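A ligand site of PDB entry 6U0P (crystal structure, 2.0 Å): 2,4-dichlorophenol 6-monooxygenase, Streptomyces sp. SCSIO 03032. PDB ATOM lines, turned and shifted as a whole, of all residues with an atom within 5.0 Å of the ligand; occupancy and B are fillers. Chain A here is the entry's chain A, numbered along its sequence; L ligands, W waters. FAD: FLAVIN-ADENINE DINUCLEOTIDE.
O of Phe 154 lies within hydrogen-bond range of N6A of the ligand, 2.9 Å away.
OD1 of Asp 319 sits at hydrogen-bond distance from O3' of the ligand (2.7 Å).
The backbone NH (N) of Asp 319 sits at hydrogen-bond distance from an oxygen (O2P) of the ligand.
The side-chain amide oxygen of Asn 45 is in hydrogen-bond range of an oxygen (O3B) of the ligand.
The side-chain amide oxygen (OE1) of Gln 129 lies within hydrogen-bond range of an oxygen (O2') of the ligand.
The backbone NH of Ala 26 lies within hydrogen-bond range of an oxygen (O1P) of the ligand, at 2.9 Å.
NH2 of Arg 55 lies within salt-bridge range of O1A of the ligand, at 2.7 Å.
The backbone NH (N) of Arg 46 is in hydrogen-bond range of a nitrogen (N3A) of the ligand (3.2 Å).
The backbone NH of Phe 154 lies within hydrogen-bond range of a nitrogen (N1A) of the ligand, at 3.0 Å.
An oxygen (O2B) of the ligand sits at hydrogen-bond distance from a ring nitrogen (ND1) of His 47 (2.5 Å).
The backbone NH of Asp 188 sits at hydrogen-bond distance from the backbone carbonyl oxygen of Val 21, at 3.2 Å.
The side-chain amide oxygen of Gln 129 lies within hydrogen-bond range of the backbone NH of Ala 56 (3.1 Å).
The side-chain amide oxygen of Asn 45 is in hydrogen-bond range of the backbone NH of Gly 23 (2.7 Å).
N of Ala 320 lies close to O of Gly 189 (3.5 Å).
NE of Arg 46 lies within salt-bridge range of OE1 of Glu 153, at 3.6 Å.
The guanidinium group of Arg 55 lies close to the side-chain amide nitrogen of Gln 129, at 3.5 Å.
The backbone NH (N) of Arg 46 lies close to the backbone carbonyl oxygen (O) of His 152 (3.3 Å).
The backbone carbonyl oxygen (O) of His 47 is in hydrogen-bond range of the side-chain amide nitrogen (ND2) of Asn 45, 3.1 Å away.
The backbone nitrogen (N) of Pro 25 lies close to an oxygen (O1P) of the ligand (3.2 Å).
Residues that only touch the ligand: Val 21 (3.5 Å), Gly 22 (3.2 Å), Gly 23 (3.8 Å), Gly 24 (3.5 Å), Val 44 (3.6 Å), Ala 56 (3.6 Å), His 152 (3.8 Å), Glu 153 (3.9 Å), Ala 187 (3.4 Å), Asp 188 (3.2 Å), Gly 189 (3.6 Å), Trp 299 (3.5 Å), Gly 318 (3.5 Å), Pro 326 (3.2 Å), Gly 329 (3.996 Å), Gly 331 (3.8 Å) and Leu 332 (3.8 Å).
Hydrophobic or aromatic side chains within 4 Å of the ligand: Val 21, Pro 25, Ala 26, His 47, Ala 56, Phe 154, Trp 299 and Pro 326.
26 residues have an atom within 4 Å of the ligand: Val 21, Gly 22, Gly 23, Gly 24, Pro 25, Ala 26, Val 44, Asn 45, Arg 46, His 47, Arg 55, Ala 56, Gln 129, His 152, Glu 153, Phe 154, Ala 187, Asp 188, Gly 189, Trp 299, Gly 318, Asp 319, Pro 326, Gly 329, Gly 331 and Leu 332.
Water W6 lies within hydrogen-bond range of an oxygen (O2A) of the ligand (2.5 Å), the backbone NH (N) of Ala 190 (3.1 Å) and the side-chain carboxylate (OD2) of Asp 319 (3.3 Å).
Water W3 lies within hydrogen-bond range of an oxygen (O2) of the ligand (2.6 Å), the backbone NH of Leu 332 (2.7 Å) and the backbone NH of Gly 331 (3.0 Å).
Water W4 lies within hydrogen-bond range of an oxygen (O2) of the ligand (2.7 Å) and the backbone NH (N) of Gly 331 (3.0 Å).
Water W1 lies within hydrogen-bond range of OE1 of Glu 133 (2.7 Å), O1A of the ligand (2.9 Å) and NE2 of Gln 129 (3.4 Å).
Water W10 lies within hydrogen-bond range of ND2 of Asn 45 (3.0 Å) and O3B of the ligand (3.1 Å).
Water W5 bridges O of Pro 326 (3.1 Å) and N3 of the ligand (3.5 Å).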
ATOM      1  N   VAL A  21      -7.855   7.499 -19.223  1.00  0.00           N
ATOM      2  CA  VAL A  21      -7.868   6.970 -17.856  1.00  0.00           C
ATOM      3  C   VAL A  21      -6.563   7.366 -17.178  1.00  0.00           C
ATOM      4  O   VAL A  21      -5.533   6.804 -17.551  1.00  0.00           O
ATOM      5  CB  VAL A  21      -8.062   5.445 -17.859  1.00  0.00           C
ATOM      6  CG1 VAL A  21      -8.126   4.925 -16.447  1.00  0.00           C
ATOM      7  CG2 VAL A  21      -9.324   5.083 -18.626  1.00  0.00           C
ATOM      8  N   GLY A  22      -6.618   8.288 -16.226  1.00  0.00           N
ATOM      9  CA  GLY A  22      -5.439   8.682 -15.440  1.00  0.00           C
ATOM     10  C   GLY A  22      -5.117  10.122 -15.728  1.00  0.00           C
ATOM     11  O   GLY A  22      -5.154  10.470 -16.913  1.00  0.00           O
ATOM     12  N   GLY A  23      -4.929  10.926 -14.681  1.00  0.00           N
ATOM     13  CA  GLY A  23      -4.656  12.365 -14.800  1.00  0.00           C
ATOM     14  C   GLY A  23      -3.369  12.770 -14.086  1.00  0.00           C
ATOM     15  O   GLY A  23      -3.365  13.829 -13.465  1.00  0.00           O
ATOM     16  N   GLY A  24      -2.306  11.980 -14.211  1.00  0.00           N
ATOM     17  CA  GLY A  24      -0.934  12.391 -13.904  1.00  0.00           C
ATOM     18  C   GLY A  24      -0.404  13.085 -15.147  1.00  0.00           C
ATOM     19  O   GLY A  24      -1.157  13.341 -16.089  1.00  0.00           O
ATOM     20  N   PRO A  25       0.925  13.305 -15.246  1.00  0.00           N
ATOM     21  CA  PRO A  25       1.488  14.007 -16.401  1.00  0.00           C
ATOM     22  C   PRO A  25       1.151  13.377 -17.761  1.00  0.00           C
ATOM     23  O   PRO A  25       0.915  14.098 -18.731  1.00  0.00           O
ATOM     24  CB  PRO A  25       3.004  13.979 -16.141  1.00  0.00           C
ATOM     25  CG  PRO A  25       3.144  13.737 -14.630  1.00  0.00           C
ATOM     26  CD  PRO A  25       1.916  12.957 -14.227  1.00  0.00           C
ATOM     27  N   ALA A  26       1.147  12.059 -17.877  1.00  0.00           N
ATOM     28  CA  ALA A  26       0.869  11.448 -19.191  1.00  0.00           C
ATOM     29  C   ALA A  26      -0.580  11.767 -19.601  1.00  0.00           C
ATOM     30  O   ALA A  26      -0.813  12.289 -20.724  1.00  0.00           O
ATOM     31  CB  ALA A  26       1.175   9.964 -19.149  1.00  0.00           C
ATOM     32  N   GLY A  27      -1.561  11.511 -18.737  1.00  0.00           N
ATOM     33  CA  GLY A  27      -2.980  11.759 -19.127  1.00  0.00           C
ATOM     34  C   GLY A  27      -3.276  13.223 -19.353  1.00  0.00           C
ATOM     35  O   GLY A  27      -3.974  13.594 -20.294  1.00  0.00           O
ATOM     36  N   VAL A  44     -10.741  10.682 -16.799  1.00  0.00           N
ATOM     37  CA  VAL A  44     -11.169  10.330 -15.435  1.00  0.00           C
ATOM     38  C   VAL A  44      -9.925  10.049 -14.653  1.00  0.00           C
ATOM     39  O   VAL A  44      -9.003   9.429 -15.196  1.00  0.00           O
ATOM     40  CB  VAL A  44     -12.155   9.135 -15.434  1.00  0.00           C
ATOM     41  CG1 VAL A  44     -13.419   9.481 -16.194  1.00  0.00           C
ATOM     42  CG2 VAL A  44     -11.503   7.860 -16.006  1.00  0.00           C
ATOM     43  N   ASN A  45      -9.910  10.481 -13.416  1.00  0.00           N
ATOM     44  CA  ASN A  45      -8.738  10.297 -12.543  1.00  0.00           C
ATOM     45  C   ASN A  45      -9.276   9.857 -11.205  1.00  0.00           C
ATOM     46  O   ASN A  45     -10.196  10.539 -10.713  1.00  0.00           O
ATOM     47  CB  ASN A  45      -7.945  11.602 -12.342  1.00  0.00           C
ATOM     48  CG  ASN A  45      -6.702  11.352 -11.542  1.00  0.00           C
ATOM     49  OD1 ASN A  45      -5.743  10.809 -12.085  1.00  0.00           O
ATOM     50  ND2 ASN A  45      -6.707  11.652 -10.243  1.00  0.00           N
ATOM     51  N   ARG A  46      -8.718   8.817 -10.610  1.00  0.00           N
ATOM     52  CA  ARG A  46      -9.397   8.170  -9.460  1.00  0.00           C
ATOM     53  C   ARG A  46      -9.226   9.045  -8.222  1.00  0.00           C
ATOM     54  O   ARG A  46     -10.143   9.082  -7.417  1.00  0.00           O
ATOM     55  CB  ARG A  46      -8.970   6.729  -9.260  1.00  0.00           C
ATOM     56  CG  ARG A  46      -7.581   6.519  -8.701  1.00  0.00           C
ATOM     57  CD  ARG A  46      -7.371   5.026  -8.449  1.00  0.00           C
ATOM     58  NE  ARG A  46      -8.084   4.648  -7.239  1.00  0.00           N
ATOM     59  CZ  ARG A  46      -7.596   4.764  -6.004  1.00  0.00           C
ATOM     60  NH1 ARG A  46      -6.368   5.214  -5.801  1.00  0.00           N
ATOM     61  NH2 ARG A  46      -8.337   4.400  -4.962  1.00  0.00           N
ATOM     62  N   HIS A  47      -8.077   9.706  -8.042  1.00  0.00           N
ATOM     63  CA  HIS A  47      -7.824  10.542  -6.846  1.00  0.00           C
ATOM     64  C   HIS A  47      -8.616  11.830  -6.981  1.00  0.00           C
ATOM     65  O   HIS A  47      -8.896  12.257  -8.141  1.00  0.00           O
ATOM     66  CB  HIS A  47      -6.321  10.811  -6.639  1.00  0.00           C
ATOM     67  CG  HIS A  47      -5.533   9.634  -6.163  1.00  0.00           C
ATOM     68  ND1 HIS A  47      -4.711   8.922  -7.002  1.00  0.00           N
ATOM     69  CD2 HIS A  47      -5.402   9.091  -4.933  1.00  0.00           C
ATOM     70  CE1 HIS A  47      -4.120   7.959  -6.317  1.00  0.00           C
ATOM     71  NE2 HIS A  47      -4.523   8.043  -5.056  1.00  0.00           N
ATOM     72  N   ARG A  55       7.343  14.131  -6.119  1.00  0.00           N
ATOM     73  CA  ARG A  55       7.589  13.014  -7.083  1.00  0.00           C
ATOM     74  C   ARG A  55       8.637  13.489  -8.098  1.00  0.00           C
ATOM     75  O   ARG A  55       9.650  14.035  -7.638  1.00  0.00           O
ATOM     76  CB  ARG A  55       6.253  12.586  -7.668  1.00  0.00           C
ATOM     77  CG  ARG A  55       5.338  12.079  -6.560  1.00  0.00           C
ATOM     78  CD  ARG A  55       4.073  11.380  -6.993  1.00  0.00           C
ATOM     79  NE  ARG A  55       4.049  10.866  -8.349  1.00  0.00           N
ATOM     80  CZ  ARG A  55       3.217   9.926  -8.772  1.00  0.00           C
ATOM     81  NH1 ARG A  55       2.384   9.355  -7.910  1.00  0.00           N
ATOM     82  NH2 ARG A  55       3.251   9.541 -10.038  1.00  0.00           N
ATOM     83  N   ALA A  56       8.363  13.371  -9.384  1.00  0.00           N
ATOM     84  CA  ALA A  56       9.304  13.693 -10.495  1.00  0.00           C
ATOM     85  C   ALA A  56       9.321  15.194 -10.742  1.00  0.00           C
ATOM     86  O   ALA A  56       8.226  15.820 -10.683  1.00  0.00           O
ATOM     87  CB  ALA A  56       8.894  12.982 -11.749  1.00  0.00           C
ATOM     88  N   HIS A  57      10.504  15.721 -11.055  1.00  0.00           N
ATOM     89  CA  HIS A  57      10.792  17.177 -11.021  1.00  0.00           C
ATOM     90  C   HIS A  57      11.675  17.621 -12.202  1.00  0.00           C
ATOM     91  O   HIS A  57      11.476  18.748 -12.685  1.00  0.00           O
ATOM     92  CB  HIS A  57      11.371  17.524  -9.640  1.00  0.00           C
ATOM     93  CG  HIS A  57      12.478  16.633  -9.213  1.00  0.00           C
ATOM     94  ND1 HIS A  57      13.794  16.843  -9.576  1.00  0.00           N
ATOM     95  CD2 HIS A  57      12.481  15.507  -8.455  1.00  0.00           C
ATOM     96  CE1 HIS A  57      14.542  15.899  -9.036  1.00  0.00           C
ATOM     97  NE2 HIS A  57      13.770  15.078  -8.357  1.00  0.00           N
ATOM     98  N   GLN A 129       5.855  17.779  -9.480  1.00  0.00           N
ATOM     99  CA  GLN A 129       4.548  17.368 -10.071  1.00  0.00           C
ATOM    100  C   GLN A 129       3.403  18.088  -9.372  1.00  0.00           C
ATOM    101  O   GLN A 129       2.395  18.381 -10.054  1.00  0.00           O
ATOM    102  CB  GLN A 129       4.327  15.856  -9.932  1.00  0.00           C
ATOM    103  CG  GLN A 129       4.912  15.062 -11.079  1.00  0.00           C
ATOM    104  CD  GLN A 129       4.718  13.568 -10.885  1.00  0.00           C
ATOM    105  OE1 GLN A 129       5.685  12.816 -10.764  1.00  0.00           O
ATOM    106  NE2 GLN A 129       3.461  13.133 -10.886  1.00  0.00           N
ATOM    107  N   GLU A 133       1.178  19.633 -12.346  1.00  0.00           N
ATOM    108  CA  GLU A 133      -0.142  19.055 -12.704  1.00  0.00           C
ATOM    109  C   GLU A 133      -1.224  20.122 -12.656  1.00  0.00           C
ATOM    110  O   GLU A 133      -2.050  20.178 -13.560  1.00  0.00           O
ATOM    111  CB  GLU A 133      -0.462  17.850 -11.824  1.00  0.00           C
ATOM    112  CG  GLU A 133       0.433  16.662 -12.111  1.00  0.00           C
ATOM    113  CD  GLU A 133       0.199  15.470 -11.201  1.00  0.00           C
ATOM    114  OE1 GLU A 133       1.053  14.529 -11.243  1.00  0.00           O
ATOM    115  OE2 GLU A 133      -0.874  15.472 -10.462  1.00  0.00           O
ATOM    116  N   HIS A 152     -13.212   9.959 -10.109  1.00  0.00           N
ATOM    117  CA  HIS A 152     -13.863   8.947 -10.990  1.00  0.00           C
ATOM    118  C   HIS A 152     -12.878   7.809 -11.325  1.00  0.00           C
ATOM    119  O   HIS A 152     -11.744   8.084 -11.799  1.00  0.00           O
ATOM    120  CB  HIS A 152     -14.454   9.588 -12.243  1.00  0.00           C
ATOM    121  CG  HIS A 152     -15.634  10.435 -11.931  1.00  0.00           C
ATOM    122  ND1 HIS A 152     -16.854  10.234 -12.532  1.00  0.00           N
ATOM    123  CD2 HIS A 152     -15.794  11.432 -11.021  1.00  0.00           C
ATOM    124  CE1 HIS A 152     -17.733  11.092 -12.035  1.00  0.00           C
ATOM    125  NE2 HIS A 152     -17.111  11.835 -11.094  1.00  0.00           N
ATOM    126  N   GLU A 153     -13.285   6.561 -11.084  1.00  0.00           N
ATOM    127  CA  GLU A 153     -12.394   5.381 -11.154  1.00  0.00           C
ATOM    128  C   GLU A 153     -12.797   4.501 -12.352  1.00  0.00           C
ATOM    129  O   GLU A 153     -13.999   4.102 -12.481  1.00  0.00           O
ATOM    130  CB  GLU A 153     -12.429   4.667  -9.828  1.00  0.00           C
ATOM    131  CG  GLU A 153     -11.642   3.365  -9.827  1.00  0.00           C
ATOM    132  CD  GLU A 153     -11.207   2.957  -8.441  1.00  0.00           C
ATOM    133  OE1 GLU A 153     -11.584   3.650  -7.497  1.00  0.00           O
ATOM    134  OE2 GLU A 153     -10.479   1.967  -8.307  1.00  0.00           O
ATOM    135  N   PHE A 154     -11.831   4.229 -13.223  1.00  0.00           N
ATOM    136  CA  PHE A 154     -11.964   3.210 -14.284  1.00  0.00           C
ATOM    137  C   PHE A 154     -12.028   1.818 -13.647  1.00  0.00           C
ATOM    138  O   PHE A 154     -11.175   1.537 -12.787  1.00  0.00           O
ATOM    139  CB  PHE A 154     -10.817   3.322 -15.272  1.00  0.00           C
ATOM    140  CG  PHE A 154     -10.783   2.167 -16.227  1.00  0.00           C
ATOM    141  CD1 PHE A 154     -11.472   2.211 -17.429  1.00  0.00           C
ATOM    142  CD2 PHE A 154     -10.089   1.020 -15.898  1.00  0.00           C
ATOM    143  CE1 PHE A 154     -11.451   1.132 -18.289  1.00  0.00           C
ATOM    144  CE2 PHE A 154     -10.039  -0.057 -16.781  1.00  0.00           C
ATOM    145  CZ  PHE A 154     -10.711   0.018 -17.976  1.00  0.00           C
ATOM    146  N   ALA A 187      -3.463   5.926 -19.169  1.00  0.00           N
ATOM    147  CA  ALA A 187      -2.497   6.856 -18.541  1.00  0.00           C
ATOM    148  C   ALA A 187      -2.593   6.705 -17.034  1.00  0.00           C
ATOM    149  O   ALA A 187      -2.438   7.738 -16.310  1.00  0.00           O
ATOM    150  CB  ALA A 187      -2.769   8.262 -18.988  1.00  0.00           C
ATOM    151  N   ASP A 188      -2.782   5.476 -16.555  1.00  0.00           N
ATOM    152  CA  ASP A 188      -3.210   5.235 -15.146  1.00  0.00           C
ATOM    153  C   ASP A 188      -2.048   4.844 -14.246  1.00  0.00           C
ATOM    154  O   ASP A 188      -2.281   4.461 -13.117  1.00  0.00           O
ATOM    155  CB  ASP A 188      -4.424   4.276 -15.023  1.00  0.00           C
ATOM    156  CG  ASP A 188      -4.375   2.948 -15.790  1.00  0.00           C
ATOM    157  OD1 ASP A 188      -3.611   2.837 -16.836  1.00  0.00           O
ATOM    158  OD2 ASP A 188      -5.145   2.025 -15.370  1.00  0.00           O
ATOM    159  N   GLY A 189      -0.798   4.977 -14.690  1.00  0.00           N
ATOM    160  CA  GLY A 189       0.339   4.825 -13.759  1.00  0.00           C
ATOM    161  C   GLY A 189       0.765   3.393 -13.609  1.00  0.00           C
ATOM    162  O   GLY A 189       0.221   2.525 -14.315  1.00  0.00           O
ATOM    163  N   ALA A 190       1.770   3.172 -12.761  1.00  0.00           N
ATOM    164  CA  ALA A 190       2.295   1.856 -12.350  1.00  0.00           C
ATOM    165  C   ALA A 190       1.108   0.985 -11.933  1.00  0.00           C
ATOM    166  O   ALA A 190       0.195   1.530 -11.291  1.00  0.00           O
ATOM    167  CB  ALA A 190       3.279   2.046 -11.197  1.00  0.00           C
ATOM    168  N   ARG A 193      -4.329  -0.753 -14.302  1.00  0.00           N
ATOM    169  CA  ARG A 193      -5.514  -1.601 -14.497  1.00  0.00           C
ATOM    170  C   ARG A 193      -5.836  -1.672 -15.993  1.00  0.00           C
ATOM    171  O   ARG A 193      -6.236  -2.743 -16.463  1.00  0.00           O
ATOM    172  CB  ARG A 193      -6.670  -1.088 -13.637  1.00  0.00           C
ATOM    173  CG  ARG A 193      -8.037  -1.572 -14.096  1.00  0.00           C
ATOM    174  CD  ARG A 193      -8.939  -2.156 -13.009  1.00  0.00           C
ATOM    175  NE  ARG A 193      -9.106  -1.353 -11.806  1.00  0.00           N
ATOM    176  CZ  ARG A 193      -8.600  -1.631 -10.607  1.00  0.00           C
ATOM    177  NH1 ARG A 193      -8.856  -0.839  -9.580  1.00  0.00           N
ATOM    178  NH2 ARG A 193      -7.846  -2.704 -10.411  1.00  0.00           N
ATOM    179  N   ALA A 298       6.980   6.279   1.322  1.00  0.00           N
ATOM    180  CA  ALA A 298       7.679   5.060   0.878  1.00  0.00           C
ATOM    181  C   ALA A 298       7.184   4.758  -0.527  1.00  0.00           C
ATOM    182  O   ALA A 298       6.030   5.082  -0.862  1.00  0.00           O
ATOM    183  CB  ALA A 298       7.439   3.902   1.824  1.00  0.00           C
ATOM    184  N   TRP A 299       8.063   4.215  -1.337  1.00  0.00           N
ATOM    185  CA  TRP A 299       7.836   4.019  -2.787  1.00  0.00           C
ATOM    186  C   TRP A 299       8.550   2.722  -3.179  1.00  0.00           C
ATOM    187  O   TRP A 299       9.643   2.451  -2.651  1.00  0.00           O
ATOM    188  CB  TRP A 299       8.337   5.277  -3.518  1.00  0.00           C
ATOM    189  CG  TRP A 299       8.397   5.155  -5.015  1.00  0.00           C
ATOM    190  CD1 TRP A 299       7.556   4.440  -5.819  1.00  0.00           C
ATOM    191  CD2 TRP A 299       9.367   5.777  -5.886  1.00  0.00           C
ATOM    192  NE1 TRP A 299       7.939   4.569  -7.134  1.00  0.00           N
ATOM    193  CE2 TRP A 299       9.042   5.386  -7.209  1.00  0.00           C
ATOM    194  CE3 TRP A 299      10.468   6.634  -5.682  1.00  0.00           C
ATOM    195  CZ2 TRP A 299       9.771   5.818  -8.313  1.00  0.00           C
ATOM    196  CZ3 TRP A 299      11.195   7.052  -6.772  1.00  0.00           C
ATOM    197  CH2 TRP A 299      10.850   6.655  -8.076  1.00  0.00           C
ATOM    198  N   VAL A 317       0.305   4.745 -22.093  1.00  0.00           N
ATOM    199  CA  VAL A 317       1.356   5.799 -22.041  1.00  0.00           C
ATOM    200  C   VAL A 317       1.982   5.840 -20.669  1.00  0.00           C
ATOM    201  O   VAL A 317       1.326   5.521 -19.682  1.00  0.00           O
ATOM    202  CB  VAL A 317       0.822   7.205 -22.371  1.00  0.00           C
ATOM    203  CG1 VAL A 317       0.425   7.328 -23.821  1.00  0.00           C
ATOM    204  CG2 VAL A 317      -0.303   7.633 -21.436  1.00  0.00           C
ATOM    205  N   GLY A 318       3.204   6.371 -20.601  1.00  0.00           N
ATOM    206  CA  GLY A 318       3.808   6.769 -19.324  1.00  0.00           C
ATOM    207  C   GLY A 318       4.109   5.593 -18.433  1.00  0.00           C
ATOM    208  O   GLY A 318       4.581   4.555 -18.916  1.00  0.00           O
ATOM    209  N   ASP A 319       3.895   5.782 -17.144  1.00  0.00           N
ATOM    210  CA  ASP A 319       4.236   4.776 -16.108  1.00  0.00           C
ATOM    211  C   ASP A 319       3.417   3.475 -16.249  1.00  0.00           C
ATOM    212  O   ASP A 319       3.858   2.428 -15.682  1.00  0.00           O
ATOM    213  CB  ASP A 319       4.093   5.371 -14.709  1.00  0.00           C
ATOM    214  CG  ASP A 319       5.398   5.932 -14.165  1.00  0.00           C
ATOM    215  OD1 ASP A 319       6.224   6.404 -14.972  1.00  0.00           O
ATOM    216  OD2 ASP A 319       5.594   5.852 -12.928  1.00  0.00           O
ATOM    217  N   ALA A 320       2.295   3.501 -16.957  1.00  0.00           N
ATOM    218  CA  ALA A 320       1.556   2.257 -17.321  1.00  0.00           C
ATOM    219  C   ALA A 320       2.486   1.263 -18.057  1.00  0.00           C
ATOM    220  O   ALA A 320       2.330   0.027 -17.846  1.00  0.00           O
ATOM    221  CB  ALA A 320       0.347   2.584 -18.165  1.00  0.00           C
ATOM    222  N   PRO A 326      14.436   6.653 -10.074  1.00  0.00           N
ATOM    223  CA  PRO A 326      14.393   8.081 -10.426  1.00  0.00           C
ATOM    224  C   PRO A 326      15.672   8.593 -11.153  1.00  0.00           C
ATOM    225  O   PRO A 326      15.544   9.551 -11.906  1.00  0.00           O
ATOM    226  CB  PRO A 326      14.138   8.715  -9.036  1.00  0.00           C
ATOM    227  CG  PRO A 326      14.861   7.782  -8.073  1.00  0.00           C
ATOM    228  CD  PRO A 326      14.514   6.402  -8.629  1.00  0.00           C
ATOM    229  N   GLY A 329      15.846  10.797 -14.403  1.00  0.00           N
ATOM    230  CA  GLY A 329      14.597  11.584 -14.449  1.00  0.00           C
ATOM    231  C   GLY A 329      13.945  11.453 -15.804  1.00  0.00           C
ATOM    232  O   GLY A 329      13.411  12.443 -16.360  1.00  0.00           O
ATOM    233  N   GLY A 331      11.501   9.213 -16.585  1.00  0.00           N
ATOM    234  CA  GLY A 331      10.087   8.774 -16.426  1.00  0.00           C
ATOM    235  C   GLY A 331       9.075   9.855 -16.809  1.00  0.00           C
ATOM    236  O   GLY A 331       8.312   9.652 -17.773  1.00  0.00           O
ATOM    237  N   LEU A 332       9.078  10.993 -16.132  1.00  0.00           N
ATOM    238  CA  LEU A 332       8.144  12.099 -16.460  1.00  0.00           C
ATOM    239  C   LEU A 332       8.316  12.582 -17.906  1.00  0.00           C
ATOM    240  O   LEU A 332       7.344  12.708 -18.657  1.00  0.00           O
ATOM    241  CB  LEU A 332       8.423  13.212 -15.448  1.00  0.00           C
ATOM    242  CG  LEU A 332       7.559  14.464 -15.502  1.00  0.00           C
ATOM    243  CD1 LEU A 332       7.906  15.334 -16.678  1.00  0.00           C
ATOM    244  CD2 LEU A 332       6.095  14.122 -15.559  1.00  0.00           C
ATOM    245  N   ALA A 335       6.917  10.173 -20.366  1.00  0.00           N
ATOM    246  CA  ALA A 335       5.429  10.141 -20.287  1.00  0.00           C
ATOM    247  C   ALA A 335       4.873  11.228 -21.186  1.00  0.00           C
ATOM    248  O   ALA A 335       3.932  10.986 -22.002  1.00  0.00           O
ATOM    249  CB  ALA A 335       4.937  10.315 -18.871  1.00  0.00           C
HETATM  250  PA  FAD L   1       1.030   8.773 -12.570  1.00  0.00           P
HETATM  251  O1A FAD L   1       1.717  10.089 -12.153  1.00  0.00           O
HETATM  252  O2A FAD L   1       1.372   7.710 -11.519  1.00  0.00           O
HETATM  253  O5B FAD L   1      -0.548   9.098 -12.788  1.00  0.00           O
HETATM  254  C5B FAD L   1      -1.538   8.133 -13.059  1.00  0.00           C
HETATM  255  C4B FAD L   1      -2.869   8.652 -12.520  1.00  0.00           C
HETATM  256  O4B FAD L   1      -3.904   7.724 -12.804  1.00  0.00           O
HETATM  257  C3B FAD L   1      -2.887   8.825 -11.006  1.00  0.00           C
HETATM  258  O3B FAD L   1      -3.391  10.130 -10.759  1.00  0.00           O
HETATM  259  C2B FAD L   1      -3.824   7.778 -10.423  1.00  0.00           C
HETATM  260  O2B FAD L   1      -4.790   8.293  -9.452  1.00  0.00           O
HETATM  261  C1B FAD L   1      -4.663   7.471 -11.631  1.00  0.00           C
HETATM  262  N9A FAD L   1      -5.275   6.101 -11.616  1.00  0.00           N
HETATM  263  C8A FAD L   1      -4.801   4.897 -11.168  1.00  0.00           C
HETATM  264  N7A FAD L   1      -5.789   3.961 -11.407  1.00  0.00           N
HETATM  265  C5A FAD L   1      -6.852   4.572 -12.024  1.00  0.00           C
HETATM  266  C6A FAD L   1      -8.205   4.207 -12.544  1.00  0.00           C
HETATM  267  N6A FAD L   1      -8.624   2.925 -12.460  1.00  0.00           N
HETATM  268  N1A FAD L   1      -9.010   5.218 -13.037  1.00  0.00           N
HETATM  269  C2A FAD L   1      -8.541   6.508 -13.119  1.00  0.00           C
HETATM  270  N3A FAD L   1      -7.303   6.890 -12.691  1.00  0.00           N
HETATM  271  C4A FAD L   1      -6.486   5.998 -12.125  1.00  0.00           C
HETATM  272  N1  FAD L   1       9.980   9.664 -10.724  1.00  0.00           N
HETATM  273  C2  FAD L   1      11.192  10.310 -10.712  1.00  0.00           C
HETATM  274  O2  FAD L   1      11.828  10.481 -11.788  1.00  0.00           O
HETATM  275  N3  FAD L   1      11.711  10.812  -9.560  1.00  0.00           N
HETATM  276  C4  FAD L   1      11.088  10.666  -8.381  1.00  0.00           C
HETATM  277  O4  FAD L   1      11.621  11.129  -7.371  1.00  0.00           O
HETATM  278  C4X FAD L   1       9.756   9.968  -8.293  1.00  0.00           C
HETATM  279  N5  FAD L   1       9.035   9.822  -7.131  1.00  0.00           N
HETATM  280  C5X FAD L   1       7.889   9.089  -7.166  1.00  0.00           C
HETATM  281  C6  FAD L   1       7.201   8.832  -5.983  1.00  0.00           C
HETATM  282  C7  FAD L   1       6.015   8.080  -5.973  1.00  0.00           C
HETATM  283  C7M FAD L   1       5.294   7.815  -4.671  1.00  0.00           C
HETATM  284  C8  FAD L   1       5.496   7.530  -7.264  1.00  0.00           C
HETATM  285  C8M FAD L   1       4.237   6.711  -7.338  1.00  0.00           C
HETATM  286  C9  FAD L   1       6.165   7.780  -8.457  1.00  0.00           C
HETATM  287  C9A FAD L   1       7.334   8.541  -8.462  1.00  0.00           C
HETATM  288  N10 FAD L   1       8.014   8.802  -9.671  1.00  0.00           N
HETATM  289  C10 FAD L   1       9.253   9.466  -9.605  1.00  0.00           C
HETATM  290  C1' FAD L   1       7.539   8.404 -11.014  1.00  0.00           C
HETATM  291  C2' FAD L   1       6.769   9.579 -11.606  1.00  0.00           C
HETATM  292  O2' FAD L   1       5.793  10.139 -10.693  1.00  0.00           O
HETATM  293  C3' FAD L   1       6.137   9.132 -12.897  1.00  0.00           C
HETATM  294  O3' FAD L   1       7.200   8.665 -13.754  1.00  0.00           O
HETATM  295  C4' FAD L   1       5.414  10.317 -13.501  1.00  0.00           C
HETATM  296  O4' FAD L   1       4.463  10.801 -12.546  1.00  0.00           O
HETATM  297  C5' FAD L   1       4.671  10.018 -14.816  1.00  0.00           C
HETATM  298  O5' FAD L   1       3.656   9.079 -14.514  1.00  0.00           O
HETATM  299  P   FAD L   1       2.256   8.965 -15.291  1.00  0.00           P
HETATM  300  O1P FAD L   1       1.482  10.182 -15.751  1.00  0.00           O
HETATM  301  O2P FAD L   1       2.436   7.928 -16.359  1.00  0.00           O
HETATM  302  O3P FAD L   1       1.497   8.217 -14.029  1.00  0.00           O
HETATM  303  O   HOH W   1       0.282  12.042 -10.477  1.00  0.00           O
HETATM  304  O   HOH W   2      10.727   7.031 -11.985  1.00  0.00           O
HETATM  305  O   HOH W   3      10.881  10.942 -14.173  1.00  0.00           O
HETATM  306  O   HOH W   4      12.201   8.643 -13.712  1.00  0.00           O
HETATM  307  O   HOH W   5      14.644  12.305 -10.721  1.00  0.00           O
HETATM  308  O   HOH W   6       2.758   5.647 -11.163  1.00  0.00           O
HETATM  309  O   HOH W   7      -1.789  11.317  -9.073  1.00  0.00           O
HETATM  310  O   HOH W   8       0.555   6.113 -16.980  1.00  0.00           O
HETATM  311  O   HOH W   9      -1.046  10.057 -16.241  1.00  0.00           O
HETATM  312  O   HOH W  10      -4.110  12.537  -9.026  1.00  0.00           O
